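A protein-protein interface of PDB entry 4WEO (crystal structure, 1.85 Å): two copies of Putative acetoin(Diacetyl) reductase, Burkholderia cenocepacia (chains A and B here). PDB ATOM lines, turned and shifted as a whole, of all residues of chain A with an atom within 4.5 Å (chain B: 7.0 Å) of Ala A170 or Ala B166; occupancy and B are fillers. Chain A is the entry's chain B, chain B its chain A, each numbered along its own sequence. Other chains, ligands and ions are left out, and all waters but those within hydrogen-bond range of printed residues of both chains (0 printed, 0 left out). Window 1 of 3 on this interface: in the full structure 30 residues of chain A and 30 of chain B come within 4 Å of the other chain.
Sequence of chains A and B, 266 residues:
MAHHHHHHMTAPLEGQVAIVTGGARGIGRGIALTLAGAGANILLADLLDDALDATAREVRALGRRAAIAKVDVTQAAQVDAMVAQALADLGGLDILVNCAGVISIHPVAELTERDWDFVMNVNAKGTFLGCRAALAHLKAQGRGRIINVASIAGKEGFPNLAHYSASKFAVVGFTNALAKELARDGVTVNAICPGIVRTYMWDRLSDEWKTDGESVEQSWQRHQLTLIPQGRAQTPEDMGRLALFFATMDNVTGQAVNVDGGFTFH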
ATOM      1  N   ALA A 124      23.906 -22.339   6.007  1.00  0.00           N
ATOM      2  CA  ALA A 124      23.175 -21.138   6.386  1.00  0.00           C
ATOM      3  C   ALA A 124      24.049 -20.147   7.149  1.00  0.00           C
ATOM      4  O   ALA A 124      24.186 -19.001   6.731  1.00  0.00           O
ATOM      5  CB  ALA A 124      21.942 -21.512   7.211  1.00  0.00           C
ATOM      6  N   ALA A 166      15.968 -27.524   5.512  1.00  0.00           N
ATOM      7  CA  ALA A 166      15.875 -26.466   6.507  1.00  0.00           C
ATOM      8  C   ALA A 166      16.976 -25.427   6.252  1.00  0.00           C
ATOM      9  O   ALA A 166      16.730 -24.207   6.259  1.00  0.00           O
ATOM     10  CB  ALA A 166      15.963 -27.042   7.909  1.00  0.00           C
ATOM     11  N   SER A 167      18.185 -25.912   5.990  1.00  0.00           N
ATOM     12  CA  SER A 167      19.332 -25.020   5.803  1.00  0.00           C
ATOM     13  C   SER A 167      19.201 -24.179   4.537  1.00  0.00           C
ATOM     14  O   SER A 167      19.618 -23.014   4.508  1.00  0.00           O
ATOM     15  CB  SER A 167      20.639 -25.823   5.752  1.00  0.00           C
ATOM     16  OG  SER A 167      20.840 -26.436   4.480  1.00  0.00           O
ATOM     17  N   LYS A 168      18.611 -24.757   3.492  1.00  0.00           N
ATOM     18  CA  LYS A 168      18.514 -24.063   2.213  1.00  0.00           C
ATOM     19  C   LYS A 168      17.295 -23.131   2.179  1.00  0.00           C
ATOM     20  O   LYS A 168      17.342 -22.074   1.562  1.00  0.00           O
ATOM     21  CB  LYS A 168      18.460 -25.081   1.062  1.00  0.00           C
ATOM     22  CG  LYS A 168      19.786 -25.861   0.867  1.00  0.00           C
ATOM     23  CD  LYS A 168      20.926 -24.914   0.478  1.00  0.00           C
ATOM     24  CE  LYS A 168      22.178 -25.657   0.033  1.00  0.00           C
ATOM     25  NZ  LYS A 168      23.217 -24.715  -0.496  1.00  0.00           N
ATOM     26  N   PHE A 169      16.209 -23.527   2.837  1.00  0.00           N
ATOM     27  CA  PHE A 169      15.090 -22.611   3.079  1.00  0.00           C
ATOM     28  C   PHE A 169      15.611 -21.380   3.827  1.00  0.00           C
ATOM     29  O   PHE A 169      15.258 -20.240   3.508  1.00  0.00           O
ATOM     30  CB  PHE A 169      13.981 -23.282   3.898  1.00  0.00           C
ATOM     31  CG  PHE A 169      12.908 -23.934   3.071  1.00  0.00           C
ATOM     32  CD1 PHE A 169      13.147 -25.136   2.416  1.00  0.00           C
ATOM     33  CD2 PHE A 169      11.658 -23.347   2.955  1.00  0.00           C
ATOM     34  CE1 PHE A 169      12.164 -25.733   1.656  1.00  0.00           C
ATOM     35  CE2 PHE A 169      10.659 -23.942   2.196  1.00  0.00           C
ATOM     36  CZ  PHE A 169      10.917 -25.136   1.546  1.00  0.00           C
ATOM     37  N   ALA A 170      16.447 -21.623   4.831  1.00  0.00           N
ATOM     38  CA  ALA A 170      17.061 -20.535   5.587  1.00  0.00           C
ATOM     39  C   ALA A 170      17.838 -19.585   4.682  1.00  0.00           C
ATOM     40  O   ALA A 170      17.755 -18.365   4.834  1.00  0.00           O
ATOM     41  CB  ALA A 170      17.991 -21.088   6.681  1.00  0.00           C
ATOM     42  N   VAL A 171      18.590 -20.130   3.730  1.00  0.00           N
ATOM     43  CA  VAL A 171      19.378 -19.259   2.850  1.00  0.00           C
ATOM     44  C   VAL A 171      18.456 -18.389   1.982  1.00  0.00           C
ATOM     45  O   VAL A 171      18.709 -17.202   1.780  1.00  0.00           O
ATOM     46  CB  VAL A 171      20.348 -20.059   1.974  1.00  0.00           C
ATOM     47  CG1 VAL A 171      20.993 -19.148   0.911  1.00  0.00           C
ATOM     48  CG2 VAL A 171      21.434 -20.709   2.832  1.00  0.00           C
ATOM     49  N   VAL A 172      17.378 -18.974   1.479  1.00  0.00           N
ATOM     50  CA  VAL A 172      16.404 -18.237   0.661  1.00  0.00           C
ATOM     51  C   VAL A 172      15.778 -17.068   1.436  1.00  0.00           C
ATOM     52  O   VAL A 172      15.685 -15.958   0.924  1.00  0.00           O
ATOM     53  CB  VAL A 172      15.311 -19.198   0.131  1.00  0.00           C
ATOM     54  CG1 VAL A 172      14.091 -18.444  -0.489  1.00  0.00           C
ATOM     55  CG2 VAL A 172      15.927 -20.172  -0.878  1.00  0.00           C
ATOM     56  N   GLY A 173      15.356 -17.324   2.666  1.00  0.00           N
ATOM     57  CA  GLY A 173      14.747 -16.300   3.499  1.00  0.00           C
ATOM     58  C   GLY A 173      15.753 -15.231   3.884  1.00  0.00           C
ATOM     59  O   GLY A 173      15.436 -14.043   3.876  1.00  0.00           O
ATOM     60  N   PHE A 174      16.969 -15.653   4.221  1.00  0.00           N
ATOM     61  CA  PHE A 174      18.034 -14.715   4.593  1.00  0.00           C
ATOM     62  C   PHE A 174      18.350 -13.770   3.425  1.00  0.00           C
ATOM     63  O   PHE A 174      18.515 -12.556   3.614  1.00  0.00           O
ATOM     64  CB  PHE A 174      19.283 -15.490   5.022  1.00  0.00           C
ATOM     65  CG  PHE A 174      20.446 -14.617   5.385  1.00  0.00           C
ATOM     66  CD1 PHE A 174      20.529 -14.026   6.643  1.00  0.00           C
ATOM     67  CD2 PHE A 174      21.448 -14.375   4.460  1.00  0.00           C
ATOM     68  CE1 PHE A 174      21.610 -13.201   6.976  1.00  0.00           C
ATOM     69  CE2 PHE A 174      22.532 -13.546   4.782  1.00  0.00           C
ATOM     70  CZ  PHE A 174      22.605 -12.962   6.048  1.00  0.00           C
ATOM     71  N   TRP B 116      22.559 -14.923  15.950  1.00  0.00           N
ATOM     72  CA  TRP B 116      22.224 -15.912  14.935  1.00  0.00           C
ATOM     73  C   TRP B 116      21.942 -17.281  15.560  1.00  0.00           C
ATOM     74  O   TRP B 116      20.900 -17.901  15.314  1.00  0.00           O
ATOM     75  CB  TRP B 116      23.353 -16.024  13.905  1.00  0.00           C
ATOM     76  CG  TRP B 116      23.120 -17.115  12.916  1.00  0.00           C
ATOM     77  CD1 TRP B 116      23.455 -18.429  13.047  1.00  0.00           C
ATOM     78  CD2 TRP B 116      22.489 -16.986  11.638  1.00  0.00           C
ATOM     79  NE1 TRP B 116      23.068 -19.129  11.933  1.00  0.00           N
ATOM     80  CE2 TRP B 116      22.474 -18.266  11.051  1.00  0.00           C
ATOM     81  CE3 TRP B 116      21.938 -15.909  10.930  1.00  0.00           C
ATOM     82  CZ2 TRP B 116      21.935 -18.502   9.790  1.00  0.00           C
ATOM     83  CZ3 TRP B 116      21.407 -16.146   9.673  1.00  0.00           C
ATOM     84  CH2 TRP B 116      21.409 -17.433   9.120  1.00  0.00           C
ATOM     85  N   VAL B 119      18.616 -17.577  17.839  1.00  0.00           N
ATOM     86  CA  VAL B 119      17.368 -17.681  17.121  1.00  0.00           C
ATOM     87  C   VAL B 119      17.295 -18.989  16.342  1.00  0.00           C
ATOM     88  O   VAL B 119      16.259 -19.653  16.337  1.00  0.00           O
ATOM     89  CB  VAL B 119      17.181 -16.483  16.186  1.00  0.00           C
ATOM     90  CG1 VAL B 119      16.016 -16.701  15.272  1.00  0.00           C
ATOM     91  CG2 VAL B 119      16.993 -15.217  17.011  1.00  0.00           C
ATOM     92  N   MET B 120      18.396 -19.374  15.709  1.00  0.00           N
ATOM     93  CA  MET B 120      18.392 -20.606  14.926  1.00  0.00           C
ATOM     94  C   MET B 120      18.264 -21.843  15.816  1.00  0.00           C
ATOM     95  O   MET B 120      17.528 -22.769  15.484  1.00  0.00           O
ATOM     96  CB  MET B 120      19.649 -20.712  14.066  1.00  0.00           C
ATOM     97  CG  MET B 120      19.577 -21.827  13.025  1.00  0.00           C
ATOM     98  SD  MET B 120      18.275 -21.498  11.802  1.00  0.00           S
ATOM     99  CE  MET B 120      18.692 -19.784  11.444  1.00  0.00           C
ATOM    100  N   ALA B 124      14.577 -23.160  15.111  1.00  0.00           N
ATOM    101  CA  ALA B 124      14.712 -24.224  14.127  1.00  0.00           C
ATOM    102  C   ALA B 124      15.229 -25.528  14.745  1.00  0.00           C
ATOM    103  O   ALA B 124      14.581 -26.566  14.643  1.00  0.00           O
ATOM    104  CB  ALA B 124      15.638 -23.770  12.981  1.00  0.00           C
ATOM    105  N   ALA B 153       7.264 -14.476   8.781  1.00  0.00           N
ATOM    106  CA  ALA B 153       8.670 -14.235   8.503  1.00  0.00           C
ATOM    107  C   ALA B 153       9.336 -15.497   7.953  1.00  0.00           C
ATOM    108  O   ALA B 153      10.500 -15.461   7.573  1.00  0.00           O
ATOM    109  CB  ALA B 153       9.391 -13.757   9.757  1.00  0.00           C
ATOM    110  N   GLY B 154       8.594 -16.604   7.927  1.00  0.00           N
ATOM    111  CA  GLY B 154       9.044 -17.806   7.242  1.00  0.00           C
ATOM    112  C   GLY B 154       8.574 -17.871   5.798  1.00  0.00           C
ATOM    113  O   GLY B 154       8.863 -18.842   5.097  1.00  0.00           O
ATOM    114  N   GLY B 157      11.140 -12.510   3.654  1.00  0.00           N
ATOM    115  CA  GLY B 157      12.283 -12.038   4.418  1.00  0.00           C
ATOM    116  C   GLY B 157      11.978 -10.676   5.008  1.00  0.00           C
ATOM    117  O   GLY B 157      11.560  -9.762   4.290  1.00  0.00           O
ATOM    118  N   LEU B 161      15.522  -8.507  10.515  1.00  0.00           N
ATOM    119  CA  LEU B 161      15.125  -9.810  11.029  1.00  0.00           C
ATOM    120  C   LEU B 161      15.605 -10.943  10.145  1.00  0.00           C
ATOM    121  O   LEU B 161      14.922 -11.948  10.024  1.00  0.00           O
ATOM    122  CB  LEU B 161      13.605  -9.895  11.150  1.00  0.00           C
ATOM    123  CG  LEU B 161      13.041  -9.078  12.305  1.00  0.00           C
ATOM    124  CD1 LEU B 161      11.553  -9.080  12.212  1.00  0.00           C
ATOM    125  CD2 LEU B 161      13.451  -9.708  13.580  1.00  0.00           C
ATOM    126  N   ALA B 162      16.757 -10.777   9.509  1.00  0.00           N
ATOM    127  CA  ALA B 162      17.227 -11.772   8.546  1.00  0.00           C
ATOM    128  C   ALA B 162      17.508 -13.116   9.221  1.00  0.00           C
ATOM    129  O   ALA B 162      17.257 -14.173   8.651  1.00  0.00           O
ATOM    130  CB  ALA B 162      18.466 -11.256   7.811  1.00  0.00           C
ATOM    131  N   HIS B 163      18.052 -13.068  10.436  1.00  0.00           N
ATOM    132  CA  HIS B 163      18.310 -14.290  11.193  1.00  0.00           C
ATOM    133  C   HIS B 163      16.996 -14.942  11.629  1.00  0.00           C
ATOM    134  O   HIS B 163      16.874 -16.166  11.612  1.00  0.00           O
ATOM    135  CB  HIS B 163      19.194 -14.002  12.415  1.00  0.00           C
ATOM    136  CG  HIS B 163      18.604 -13.007  13.368  1.00  0.00           C
ATOM    137  ND1 HIS B 163      17.934 -11.877  12.949  1.00  0.00           N
ATOM    138  CD2 HIS B 163      18.602 -12.963  14.724  1.00  0.00           C
ATOM    139  CE1 HIS B 163      17.533 -11.187  14.002  1.00  0.00           C
ATOM    140  NE2 HIS B 163      17.931 -11.821  15.092  1.00  0.00           N
ATOM    141  N   TYR B 164      16.027 -14.126  12.041  1.00  0.00           N
ATOM    142  CA  TYR B 164      14.719 -14.633  12.439  1.00  0.00           C
ATOM    143  C   TYR B 164      14.004 -15.252  11.245  1.00  0.00           C
ATOM    144  O   TYR B 164      13.445 -16.338  11.349  1.00  0.00           O
ATOM    145  CB  TYR B 164      13.869 -13.521  13.045  1.00  0.00           C
ATOM    146  CG  TYR B 164      12.518 -13.979  13.540  1.00  0.00           C
ATOM    147  CD1 TYR B 164      12.389 -14.627  14.769  1.00  0.00           C
ATOM    148  CD2 TYR B 164      11.366 -13.740  12.798  1.00  0.00           C
ATOM    149  CE1 TYR B 164      11.160 -15.045  15.231  1.00  0.00           C
ATOM    150  CE2 TYR B 164      10.124 -14.151  13.259  1.00  0.00           C
ATOM    151  CZ  TYR B 164      10.031 -14.805  14.475  1.00  0.00           C
ATOM    152  OH  TYR B 164       8.803 -15.220  14.928  1.00  0.00           O
ATOM    153  N   SER B 165      14.027 -14.564  10.105  1.00  0.00           N
ATOM    154  CA  SER B 165      13.480 -15.140   8.874  1.00  0.00           C
ATOM    155  C   SER B 165      14.205 -16.425   8.501  1.00  0.00           C
ATOM    156  O   SER B 165      13.565 -17.408   8.146  1.00  0.00           O
ATOM    157  CB  SER B 165      13.569 -14.153   7.696  1.00  0.00           C
ATOM    158  OG  SER B 165      12.496 -13.238   7.720  1.00  0.00           O
ATOM    159  N   ALA B 166      15.538 -16.419   8.558  1.00  0.00           N
ATOM    160  CA  ALA B 166      16.270 -17.642   8.215  1.00  0.00           C
ATOM    161  C   ALA B 166      15.739 -18.819   9.050  1.00  0.00           C
ATOM    162  O   ALA B 166      15.472 -19.913   8.525  1.00  0.00           O
ATOM    163  CB  ALA B 166      17.754 -17.462   8.437  1.00  0.00           C
ATOM    164  N   SER B 167      15.550 -18.580  10.347  1.00  0.00           N
ATOM    165  CA  SER B 167      15.108 -19.646  11.256  1.00  0.00           C
ATOM    166  C   SER B 167      13.680 -20.100  10.983  1.00  0.00           C
ATOM    167  O   SER B 167      13.368 -21.283  11.124  1.00  0.00           O
ATOM    168  CB  SER B 167      15.254 -19.203  12.732  1.00  0.00           C
ATOM    169  OG  SER B 167      14.189 -18.347  13.155  1.00  0.00           O
ATOM    170  N   LYS B 168      12.806 -19.180  10.574  1.00  0.00           N
ATOM    171  CA  LYS B 168      11.404 -19.531  10.371  1.00  0.00           C
ATOM    172  C   LYS B 168      11.177 -20.134   8.967  1.00  0.00           C
ATOM    173  O   LYS B 168      10.355 -21.028   8.799  1.00  0.00           O
ATOM    174  CB  LYS B 168      10.523 -18.295  10.617  1.00  0.00           C
ATOM    175  CG  LYS B 168      10.479 -17.849  12.110  1.00  0.00           C
ATOM    176  CD  LYS B 168       9.816 -18.928  12.990  1.00  0.00           C
ATOM    177  CE  LYS B 168       9.523 -18.457  14.405  1.00  0.00           C
ATOM    178  NZ  LYS B 168       8.733 -19.471  15.193  1.00  0.00           N
ATOM    179  N   PHE B 169      11.925 -19.666   7.972  1.00  0.00           N
ATOM    180  CA  PHE B 169      11.974 -20.345   6.680  1.00  0.00           C
ATOM    181  C   PHE B 169      12.418 -21.792   6.917  1.00  0.00           C
ATOM    182  O   PHE B 169      11.845 -22.736   6.363  1.00  0.00           O
ATOM    183  CB  PHE B 169      12.960 -19.645   5.727  1.00  0.00           C
ATOM    184  CG  PHE B 169      12.340 -18.573   4.872  1.00  0.00           C
ATOM    185  CD1 PHE B 169      11.977 -17.355   5.418  1.00  0.00           C
ATOM    186  CD2 PHE B 169      12.147 -18.784   3.509  1.00  0.00           C
ATOM    187  CE1 PHE B 169      11.418 -16.359   4.629  1.00  0.00           C
ATOM    188  CE2 PHE B 169      11.587 -17.803   2.705  1.00  0.00           C
ATOM    189  CZ  PHE B 169      11.222 -16.581   3.271  1.00  0.00           C
ATOM    190  N   ALA B 170      13.445 -21.958   7.747  1.00  0.00           N
ATOM    191  CA  ALA B 170      13.929 -23.299   8.082  1.00  0.00           C
ATOM    192  C   ALA B 170      12.815 -24.151   8.651  1.00  0.00           C
ATOM    193  O   ALA B 170      12.691 -25.319   8.299  1.00  0.00           O
ATOM    194  CB  ALA B 170      15.105 -23.243   9.056  1.00  0.00           C
ATOM    195  N   VAL B 171      11.988 -23.581   9.523  1.00  0.00           N
ATOM    196  CA  VAL B 171      10.882 -24.370  10.081  1.00  0.00           C
ATOM    197  C   VAL B 171       9.875 -24.769   9.005  1.00  0.00           C
ATOM    198  O   VAL B 171       9.378 -25.910   8.981  1.00  0.00           O
ATOM    199  CB  VAL B 171      10.164 -23.608  11.225  1.00  0.00           C
ATOM    200  CG1 VAL B 171       8.926 -24.370  11.689  1.00  0.00           C
ATOM    201  CG2 VAL B 171      11.112 -23.424  12.414  1.00  0.00           C
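Ala A166 touches Ala B170, and with the chains exchanged Ala A170 touches Ala B166.
Phe B169 touches its own counterpart, Phe A169.
7 positions are printed for both chains.
Trp B116 touches Ala A124 (CZ2 to C, 3.8 Å).
Ala A166 touches Ala B170.
Phe A169 touches Phe B169.
Ala B166 touches Ala A170.
Gly A173 touches Gly B157.
CA of Gly A173 touches CE1 of Phe B169 (3.5 Å).
CZ3 of Trp B116 touches CD1 of Phe A174, at 3.8 Å.
Ala B162 touches Phe A174 (CB to CD1, 3.6 Å).
Of the 10 printed residues of chain A, 6 touch a printed residue of chain B.
Hydrophobic or aromatic side chains of chain A within 4 Å of the printed part of chain B: Ala A124, Ala A166, Phe A169, Ala A170 and Phe A174.
Along chain A the printed residues that touch a printed residue of chain B span positions 124 to 174.
Hydrophobic or aromatic side chains of chain B that line the printed part of chain A: Trp B116, Ala B162, Ala B166, Phe B169 and Ala B170.
Among the printed residues, no Asp or Glu carboxylate lies within 4 Å of a Lys or Arg side-chain nitrogen of the other chain.
Of chain B, only Ala B166 comes within 4 Å of Ala A170.
Of the printed residues of chain A, Ala B166 touches Ala A170 (3.3 Å).
Of the printed residues of chain B, Ala A166 touches Ala B170.
Printed residues of chain A within 4 Å of Ala B162: Phe A174.
Printed residues of chain A within 4 Å of Phe B169: Phe A169 and Gly A173.
Printed residues of chain A within 4 Å of Ala B170: Ala A166 (3.4 Å).
Gly B154 touches none of the printed residues of chain A.
The nearest printed residue of chain A that does not touch Gly B157 is Phe A174 (5.9 Å).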
